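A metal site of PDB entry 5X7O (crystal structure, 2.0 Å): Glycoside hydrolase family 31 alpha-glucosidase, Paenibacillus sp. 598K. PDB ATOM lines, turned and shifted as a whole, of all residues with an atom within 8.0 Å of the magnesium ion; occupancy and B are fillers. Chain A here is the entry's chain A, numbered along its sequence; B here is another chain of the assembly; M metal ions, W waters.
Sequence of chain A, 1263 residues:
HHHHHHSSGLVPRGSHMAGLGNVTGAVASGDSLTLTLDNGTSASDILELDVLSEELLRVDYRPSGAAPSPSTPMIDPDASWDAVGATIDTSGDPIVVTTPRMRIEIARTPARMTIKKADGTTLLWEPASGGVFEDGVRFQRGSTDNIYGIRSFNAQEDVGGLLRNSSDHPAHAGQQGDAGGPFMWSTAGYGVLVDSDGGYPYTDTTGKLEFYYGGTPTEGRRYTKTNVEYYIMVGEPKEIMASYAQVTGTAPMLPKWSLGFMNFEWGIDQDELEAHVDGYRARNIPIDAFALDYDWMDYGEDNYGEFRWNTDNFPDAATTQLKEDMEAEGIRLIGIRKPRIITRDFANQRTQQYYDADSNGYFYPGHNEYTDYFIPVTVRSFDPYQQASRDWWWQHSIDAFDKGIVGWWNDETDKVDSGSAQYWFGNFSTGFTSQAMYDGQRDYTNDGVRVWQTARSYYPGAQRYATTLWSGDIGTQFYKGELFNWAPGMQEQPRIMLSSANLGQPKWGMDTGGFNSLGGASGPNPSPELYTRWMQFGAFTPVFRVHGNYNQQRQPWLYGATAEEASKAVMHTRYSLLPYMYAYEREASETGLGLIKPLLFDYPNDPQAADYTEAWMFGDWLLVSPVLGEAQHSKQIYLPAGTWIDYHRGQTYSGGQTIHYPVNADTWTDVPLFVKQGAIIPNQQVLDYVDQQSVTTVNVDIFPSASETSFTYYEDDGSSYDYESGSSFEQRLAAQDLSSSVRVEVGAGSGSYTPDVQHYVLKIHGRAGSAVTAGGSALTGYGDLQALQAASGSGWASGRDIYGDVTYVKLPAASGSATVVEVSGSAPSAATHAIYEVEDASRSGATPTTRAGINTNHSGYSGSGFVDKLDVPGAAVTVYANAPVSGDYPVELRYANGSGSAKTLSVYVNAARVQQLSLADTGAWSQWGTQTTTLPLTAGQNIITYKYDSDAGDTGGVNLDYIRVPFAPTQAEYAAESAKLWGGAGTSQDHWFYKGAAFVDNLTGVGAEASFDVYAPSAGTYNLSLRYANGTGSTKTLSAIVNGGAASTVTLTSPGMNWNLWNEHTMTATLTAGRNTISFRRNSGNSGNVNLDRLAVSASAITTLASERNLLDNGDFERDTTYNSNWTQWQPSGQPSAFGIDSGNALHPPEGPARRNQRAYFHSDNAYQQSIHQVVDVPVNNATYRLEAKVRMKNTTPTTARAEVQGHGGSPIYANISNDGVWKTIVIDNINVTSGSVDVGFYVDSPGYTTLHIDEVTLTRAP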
ATOM      1  N   GLU A 265      24.235  19.480  -1.889  1.00  0.00           N
ATOM      2  CA  GLU A 265      24.709  20.045  -0.625  1.00  0.00           C
ATOM      3  C   GLU A 265      24.410  19.212   0.633  1.00  0.00           C
ATOM      4  O   GLU A 265      23.311  18.663   0.807  1.00  0.00           O
ATOM      5  CB  GLU A 265      24.142  21.465  -0.442  1.00  0.00           C
ATOM      6  CG  GLU A 265      24.842  22.256   0.682  1.00  0.00           C
ATOM      7  CD  GLU A 265      24.628  23.769   0.601  1.00  0.00           C
ATOM      8  OE1 GLU A 265      24.629  24.321  -0.532  1.00  0.00           O
ATOM      9  OE2 GLU A 265      24.519  24.410   1.663  1.00  0.00           O
ATOM     10  N   TRP A 266      25.397  19.162   1.510  1.00  0.00           N
ATOM     11  CA  TRP A 266      25.302  18.488   2.795  1.00  0.00           C
ATOM     12  C   TRP A 266      25.564  19.559   3.857  1.00  0.00           C
ATOM     13  O   TRP A 266      26.610  20.213   3.833  1.00  0.00           O
ATOM     14  CB  TRP A 266      26.339  17.366   2.859  1.00  0.00           C
ATOM     15  CG  TRP A 266      26.345  16.527   4.110  1.00  0.00           C
ATOM     16  CD1 TRP A 266      25.375  16.436   5.060  1.00  0.00           C
ATOM     17  CD2 TRP A 266      27.386  15.646   4.519  1.00  0.00           C
ATOM     18  NE1 TRP A 266      25.749  15.565   6.048  1.00  0.00           N
ATOM     19  CE2 TRP A 266      26.979  15.064   5.738  1.00  0.00           C
ATOM     20  CE3 TRP A 266      28.634  15.290   3.978  1.00  0.00           C
ATOM     21  CZ2 TRP A 266      27.775  14.139   6.432  1.00  0.00           C
ATOM     22  CZ3 TRP A 266      29.429  14.371   4.664  1.00  0.00           C
ATOM     23  CH2 TRP A 266      28.981  13.802   5.884  1.00  0.00           C
ATOM     24  N   GLY A 267      24.617  19.699   4.784  1.00  0.00           N
ATOM     25  CA  GLY A 267      24.587  20.799   5.745  1.00  0.00           C
ATOM     26  C   GLY A 267      23.694  21.879   5.192  1.00  0.00           C
ATOM     27  O   GLY A 267      24.172  22.858   4.626  1.00  0.00           O
ATOM     28  N   ILE A 268      22.388  21.694   5.358  1.00  0.00           N
ATOM     29  CA  ILE A 268      21.375  22.524   4.691  1.00  0.00           C
ATOM     30  C   ILE A 268      19.997  22.327   5.310  1.00  0.00           C
ATOM     31  O   ILE A 268      19.606  21.221   5.656  1.00  0.00           O
ATOM     32  CB  ILE A 268      21.337  22.278   3.146  1.00  0.00           C
ATOM     33  CG1 ILE A 268      20.396  23.284   2.460  1.00  0.00           C
ATOM     34  CG2 ILE A 268      20.937  20.842   2.797  1.00  0.00           C
ATOM     35  CD1 ILE A 268      20.585  23.422   0.965  1.00  0.00           C
ATOM     36  N   ASP A 269      19.261  23.427   5.454  1.00  0.00           N
ATOM     37  CA  ASP A 269      17.875  23.406   5.908  1.00  0.00           C
ATOM     38  C   ASP A 269      17.043  24.292   4.994  1.00  0.00           C
ATOM     39  O   ASP A 269      17.594  24.903   4.070  1.00  0.00           O
ATOM     40  CB  ASP A 269      17.799  23.811   7.393  1.00  0.00           C
ATOM     41  CG  ASP A 269      18.230  25.255   7.670  1.00  0.00           C
ATOM     42  OD1 ASP A 269      18.449  26.059   6.737  1.00  0.00           O
ATOM     43  OD2 ASP A 269      18.339  25.598   8.854  1.00  0.00           O
ATOM     44  N   GLU A 272      18.099  28.029   4.448  1.00  0.00           N
ATOM     45  CA  GLU A 272      19.345  28.138   3.689  1.00  0.00           C
ATOM     46  C   GLU A 272      19.122  27.779   2.204  1.00  0.00           C
ATOM     47  O   GLU A 272      19.650  28.458   1.322  1.00  0.00           O
ATOM     48  CB  GLU A 272      20.417  27.244   4.341  1.00  0.00           C
ATOM     49  CG  GLU A 272      21.808  27.263   3.732  1.00  0.00           C
ATOM     50  CD  GLU A 272      22.791  26.297   4.408  1.00  0.00           C
ATOM     51  OE1 GLU A 272      22.437  25.680   5.445  1.00  0.00           O
ATOM     52  OE2 GLU A 272      23.946  26.168   3.925  1.00  0.00           O
ATOM     53  N   LEU A 273      18.296  26.762   1.942  1.00  0.00           N
ATOM     54  CA  LEU A 273      17.931  26.379   0.575  1.00  0.00           C
ATOM     55  C   LEU A 273      17.265  27.552  -0.172  1.00  0.00           C
ATOM     56  O   LEU A 273      17.636  27.880  -1.298  1.00  0.00           O
ATOM     57  CB  LEU A 273      17.015  25.165   0.595  1.00  0.00           C
ATOM     58  CG  LEU A 273      16.355  24.761  -0.723  1.00  0.00           C
ATOM     59  CD1 LEU A 273      17.377  24.279  -1.733  1.00  0.00           C
ATOM     60  CD2 LEU A 273      15.307  23.694  -0.476  1.00  0.00           C
ATOM     61  N   HIS A 276      19.794  30.176  -0.977  1.00  0.00           N
ATOM     62  CA  HIS A 276      20.601  29.751  -2.121  1.00  0.00           C
ATOM     63  C   HIS A 276      19.880  29.999  -3.431  1.00  0.00           C
ATOM     64  O   HIS A 276      20.453  30.616  -4.326  1.00  0.00           O
ATOM     65  CB  HIS A 276      21.001  28.268  -2.053  1.00  0.00           C
ATOM     66  CG  HIS A 276      21.878  27.919  -0.895  1.00  0.00           C
ATOM     67  ND1 HIS A 276      22.686  28.852  -0.278  1.00  0.00           N
ATOM     68  CD2 HIS A 276      22.096  26.747  -0.264  1.00  0.00           C
ATOM     69  CE1 HIS A 276      23.361  28.270   0.706  1.00  0.00           C
ATOM     70  NE2 HIS A 276      23.015  26.994   0.737  1.00  0.00           N
ATOM     71  N   PHE A 290      18.387  21.239  -6.717  1.00  0.00           N
ATOM     72  CA  PHE A 290      19.190  21.051  -5.532  1.00  0.00           C
ATOM     73  C   PHE A 290      19.079  19.601  -5.115  1.00  0.00           C
ATOM     74  O   PHE A 290      17.982  19.023  -5.156  1.00  0.00           O
ATOM     75  CB  PHE A 290      18.716  21.941  -4.394  1.00  0.00           C
ATOM     76  CG  PHE A 290      19.598  23.112  -4.140  1.00  0.00           C
ATOM     77  CD1 PHE A 290      19.406  24.310  -4.816  1.00  0.00           C
ATOM     78  CD2 PHE A 290      20.647  23.009  -3.232  1.00  0.00           C
ATOM     79  CE1 PHE A 290      20.245  25.390  -4.581  1.00  0.00           C
ATOM     80  CE2 PHE A 290      21.486  24.082  -2.990  1.00  0.00           C
ATOM     81  CZ  PHE A 290      21.272  25.272  -3.658  1.00  0.00           C
ATOM     82  N   ASP A 295      20.506  15.668   5.492  1.00  0.00           N
ATOM     83  CA  ASP A 295      19.620  16.715   5.998  1.00  0.00           C
ATOM     84  C   ASP A 295      18.143  16.518   5.678  1.00  0.00           C
ATOM     85  O   ASP A 295      17.301  16.936   6.475  1.00  0.00           O
ATOM     86  CB  ASP A 295      20.055  18.095   5.470  1.00  0.00           C
ATOM     87  CG  ASP A 295      21.533  18.350   5.630  1.00  0.00           C
ATOM     88  OD1 ASP A 295      22.329  17.937   4.751  1.00  0.00           O
ATOM     89  OD2 ASP A 295      21.922  18.980   6.631  1.00  0.00           O
ATOM     90  N   ASN B 348      28.125  24.788  12.933  1.00  0.00           N
ATOM     91  CA  ASN B 348      29.262  25.295  12.137  1.00  0.00           C
ATOM     92  C   ASN B 348      29.859  26.661  12.586  1.00  0.00           C
ATOM     93  O   ASN B 348      30.607  27.277  11.833  1.00  0.00           O
ATOM     94  CB  ASN B 348      28.919  25.341  10.635  1.00  0.00           C
ATOM     95  CG  ASN B 348      30.162  25.332   9.744  1.00  0.00           C
ATOM     96  OD1 ASN B 348      31.100  24.570   9.972  1.00  0.00           O
ATOM     97  ND2 ASN B 348      30.173  26.207   8.739  1.00  0.00           N
ATOM     98  N   ASN B 549      31.887  18.880   0.697  1.00  0.00           N
ATOM     99  CA  ASN B 549      31.853  18.108   1.938  1.00  0.00           C
ATOM    100  C   ASN B 549      30.888  18.744   2.939  1.00  0.00           C
ATOM    101  O   ASN B 549      30.218  19.756   2.653  1.00  0.00           O
ATOM    102  CB  ASN B 549      33.285  17.936   2.516  1.00  0.00           C
ATOM    103  CG  ASN B 549      33.487  16.600   3.223  1.00  0.00           C
ATOM    104  OD1 ASN B 549      32.556  16.048   3.806  1.00  0.00           O
ATOM    105  ND2 ASN B 549      34.708  16.092   3.202  1.00  0.00           N
ATOM    106  N   TYR B 550      30.789  18.127   4.116  1.00  0.00           N
ATOM    107  CA  TYR B 550      29.862  18.543   5.145  1.00  0.00           C
ATOM    108  C   TYR B 550      30.026  20.012   5.494  1.00  0.00           C
ATOM    109  O   TYR B 550      31.131  20.458   5.774  1.00  0.00           O
ATOM    110  CB  TYR B 550      30.097  17.708   6.399  1.00  0.00           C
ATOM    111  CG  TYR B 550      29.197  18.109   7.542  1.00  0.00           C
ATOM    112  CD1 TYR B 550      27.817  17.975   7.434  1.00  0.00           C
ATOM    113  CD2 TYR B 550      29.735  18.659   8.702  1.00  0.00           C
ATOM    114  CE1 TYR B 550      26.979  18.338   8.481  1.00  0.00           C
ATOM    115  CE2 TYR B 550      28.906  19.026   9.751  1.00  0.00           C
ATOM    116  CZ  TYR B 550      27.532  18.868   9.623  1.00  0.00           C
ATOM    117  OH  TYR B 550      26.729  19.237  10.659  1.00  0.00           O
ATOM    118  N   ASN B 551      28.922  20.759   5.442  1.00  0.00           N
ATOM    119  CA  ASN B 551      28.905  22.212   5.737  1.00  0.00           C
ATOM    120  C   ASN B 551      29.814  23.071   4.837  1.00  0.00           C
ATOM    121  O   ASN B 551      30.105  24.228   5.187  1.00  0.00           O
ATOM    122  CB  ASN B 551      29.188  22.476   7.245  1.00  0.00           C
ATOM    123  CG  ASN B 551      27.948  22.404   8.110  1.00  0.00           C
ATOM    124  OD1 ASN B 551      26.845  22.611   7.643  1.00  0.00           O
ATOM    125  ND2 ASN B 551      28.141  22.140   9.396  1.00  0.00           N
ATOM    126  N   GLN B 552      30.252  22.546   3.696  1.00  0.00           N
ATOM    127  CA  GLN B 552      30.960  23.341   2.692  1.00  0.00           C
ATOM    128  C   GLN B 552      29.921  23.927   1.718  1.00  0.00           C
ATOM    129  O   GLN B 552      28.804  23.398   1.563  1.00  0.00           O
ATOM    130  CB  GLN B 552      31.993  22.509   1.952  1.00  0.00           C
ATOM    131  CG  GLN B 552      33.121  21.997   2.827  1.00  0.00           C
ATOM    132  CD  GLN B 552      34.254  21.382   2.025  1.00  0.00           C
ATOM    133  OE1 GLN B 552      34.030  20.960   0.886  1.00  0.00           O
ATOM    134  NE2 GLN B 552      35.455  21.301   2.610  1.00  0.00           N
ATOM    135  N   GLN B 553      30.285  25.064   1.130  1.00  0.00           N
ATOM    136  CA  GLN B 553      29.416  25.775   0.195  1.00  0.00           C
ATOM    137  C   GLN B 553      30.071  25.844  -1.176  1.00  0.00           C
ATOM    138  O   GLN B 553      31.293  26.003  -1.295  1.00  0.00           O
ATOM    139  CB  GLN B 553      29.136  27.182   0.723  1.00  0.00           C
ATOM    140  CG  GLN B 553      28.417  27.248   2.090  1.00  0.00           C
ATOM    141  CD  GLN B 553      27.090  26.505   2.148  1.00  0.00           C
ATOM    142  OE1 GLN B 553      26.773  25.870   3.168  1.00  0.00           O
ATOM    143  NE2 GLN B 553      26.304  26.581   1.076  1.00  0.00           N
ATOM    144  N   ARG B 554      29.255  25.719  -2.214  1.00  0.00           N
ATOM    145  CA  ARG B 554      29.753  25.737  -3.592  1.00  0.00           C
ATOM    146  C   ARG B 554      29.002  26.736  -4.497  1.00  0.00           C
ATOM    147  O   ARG B 554      29.068  26.638  -5.727  1.00  0.00           O
ATOM    148  CB  ARG B 554      29.694  24.313  -4.153  1.00  0.00           C
ATOM    149  CG  ARG B 554      30.664  23.327  -3.518  1.00  0.00           C
ATOM    150  CD  ARG B 554      32.090  23.546  -3.995  1.00  0.00           C
ATOM    151  NE  ARG B 554      33.001  22.529  -3.483  1.00  0.00           N
ATOM    152  CZ  ARG B 554      33.622  22.551  -2.300  1.00  0.00           C
ATOM    153  NH1 ARG B 554      33.489  23.586  -1.462  1.00  0.00           N
ATOM    154  NH2 ARG B 554      34.420  21.554  -1.970  1.00  0.00           N
ATOM    155  N   GLN B 555      28.353  27.730  -3.893  1.00  0.00           N
ATOM    156  CA  GLN B 555      27.684  28.769  -4.682  1.00  0.00           C
ATOM    157  C   GLN B 555      28.755  29.666  -5.319  1.00  0.00           C
ATOM    158  O   GLN B 555      29.725  30.037  -4.656  1.00  0.00           O
ATOM    159  CB  GLN B 555      26.694  29.561  -3.837  1.00  0.00           C
ATOM    160  CG  GLN B 555      25.445  28.781  -3.429  1.00  0.00           C
ATOM    161  CD  GLN B 555      25.665  27.787  -2.288  1.00  0.00           C
ATOM    162  OE1 GLN B 555      26.440  28.046  -1.358  1.00  0.00           O
ATOM    163  NE2 GLN B 555      24.991  26.642  -2.366  1.00  0.00           N
HETATM  164 MG    MG M   1      25.266  24.491   3.830  1.00  0.00          MG
HETATM  165  O   HOH W   1      26.084  24.726   5.657  1.00  0.00           O
HETATM  166  O   HOH W   2      26.819  23.085   3.400  1.00  0.00           O
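Four residues have an atom within 4 Å of the magnesium ion: Glu 265, Gly 267, Glu 272 and Gln 553 of chain B. The nearest printed residue that does not touch the magnesium ion is Ile 268 (4.3 Å).
A ring nitrogen (ND1) of His 276 sits close to the backbone carbonyl oxygen (O) of Glu 272, 3.5 Å away. The backbone NH (N) of Glu 272 sits at hydrogen-bond distance from the side-chain carboxylate (OD1) of Asp 269, at 3.0 Å. The side-chain carboxylate of Asp 295 lies within hydrogen-bond range of the backbone NH of Gly 267, 2.9 Å away. The side-chain amide oxygen of Gln 555 of chain B sits at hydrogen-bond distance from the side-chain amide nitrogen of Gln 553 of chain B (2.8 Å). The side-chain amide nitrogen of Gln 553 of chain B sits at hydrogen-bond distance from a ring nitrogen (NE2) of His 276, 3.3 Å away. OE1 of Glu 265 is in hydrogen-bond range of NE2 of Gln 555 of chain B (3.0 Å). NE2 of His 276 sits at hydrogen-bond distance from OE1 of Glu 265 (3.4 Å).
Water W1 is bound to the magnesium ion, at 2.0 Å. O of Gly 267 binds the magnesium ion. OE2 of Glu 272 binds the magnesium ion, at 2.1 Å. The magnesium ion is bound by water W2 (2.1 Å). OE1 of Gln 553 of chain B binds the magnesium ion (2.1 Å). OE2 of Glu 265 binds the magnesium ion.
Water W2 lies within hydrogen-bond range of O of Gln 552 of chain B (2.7 Å) and O of Trp 266 (2.9 Å).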
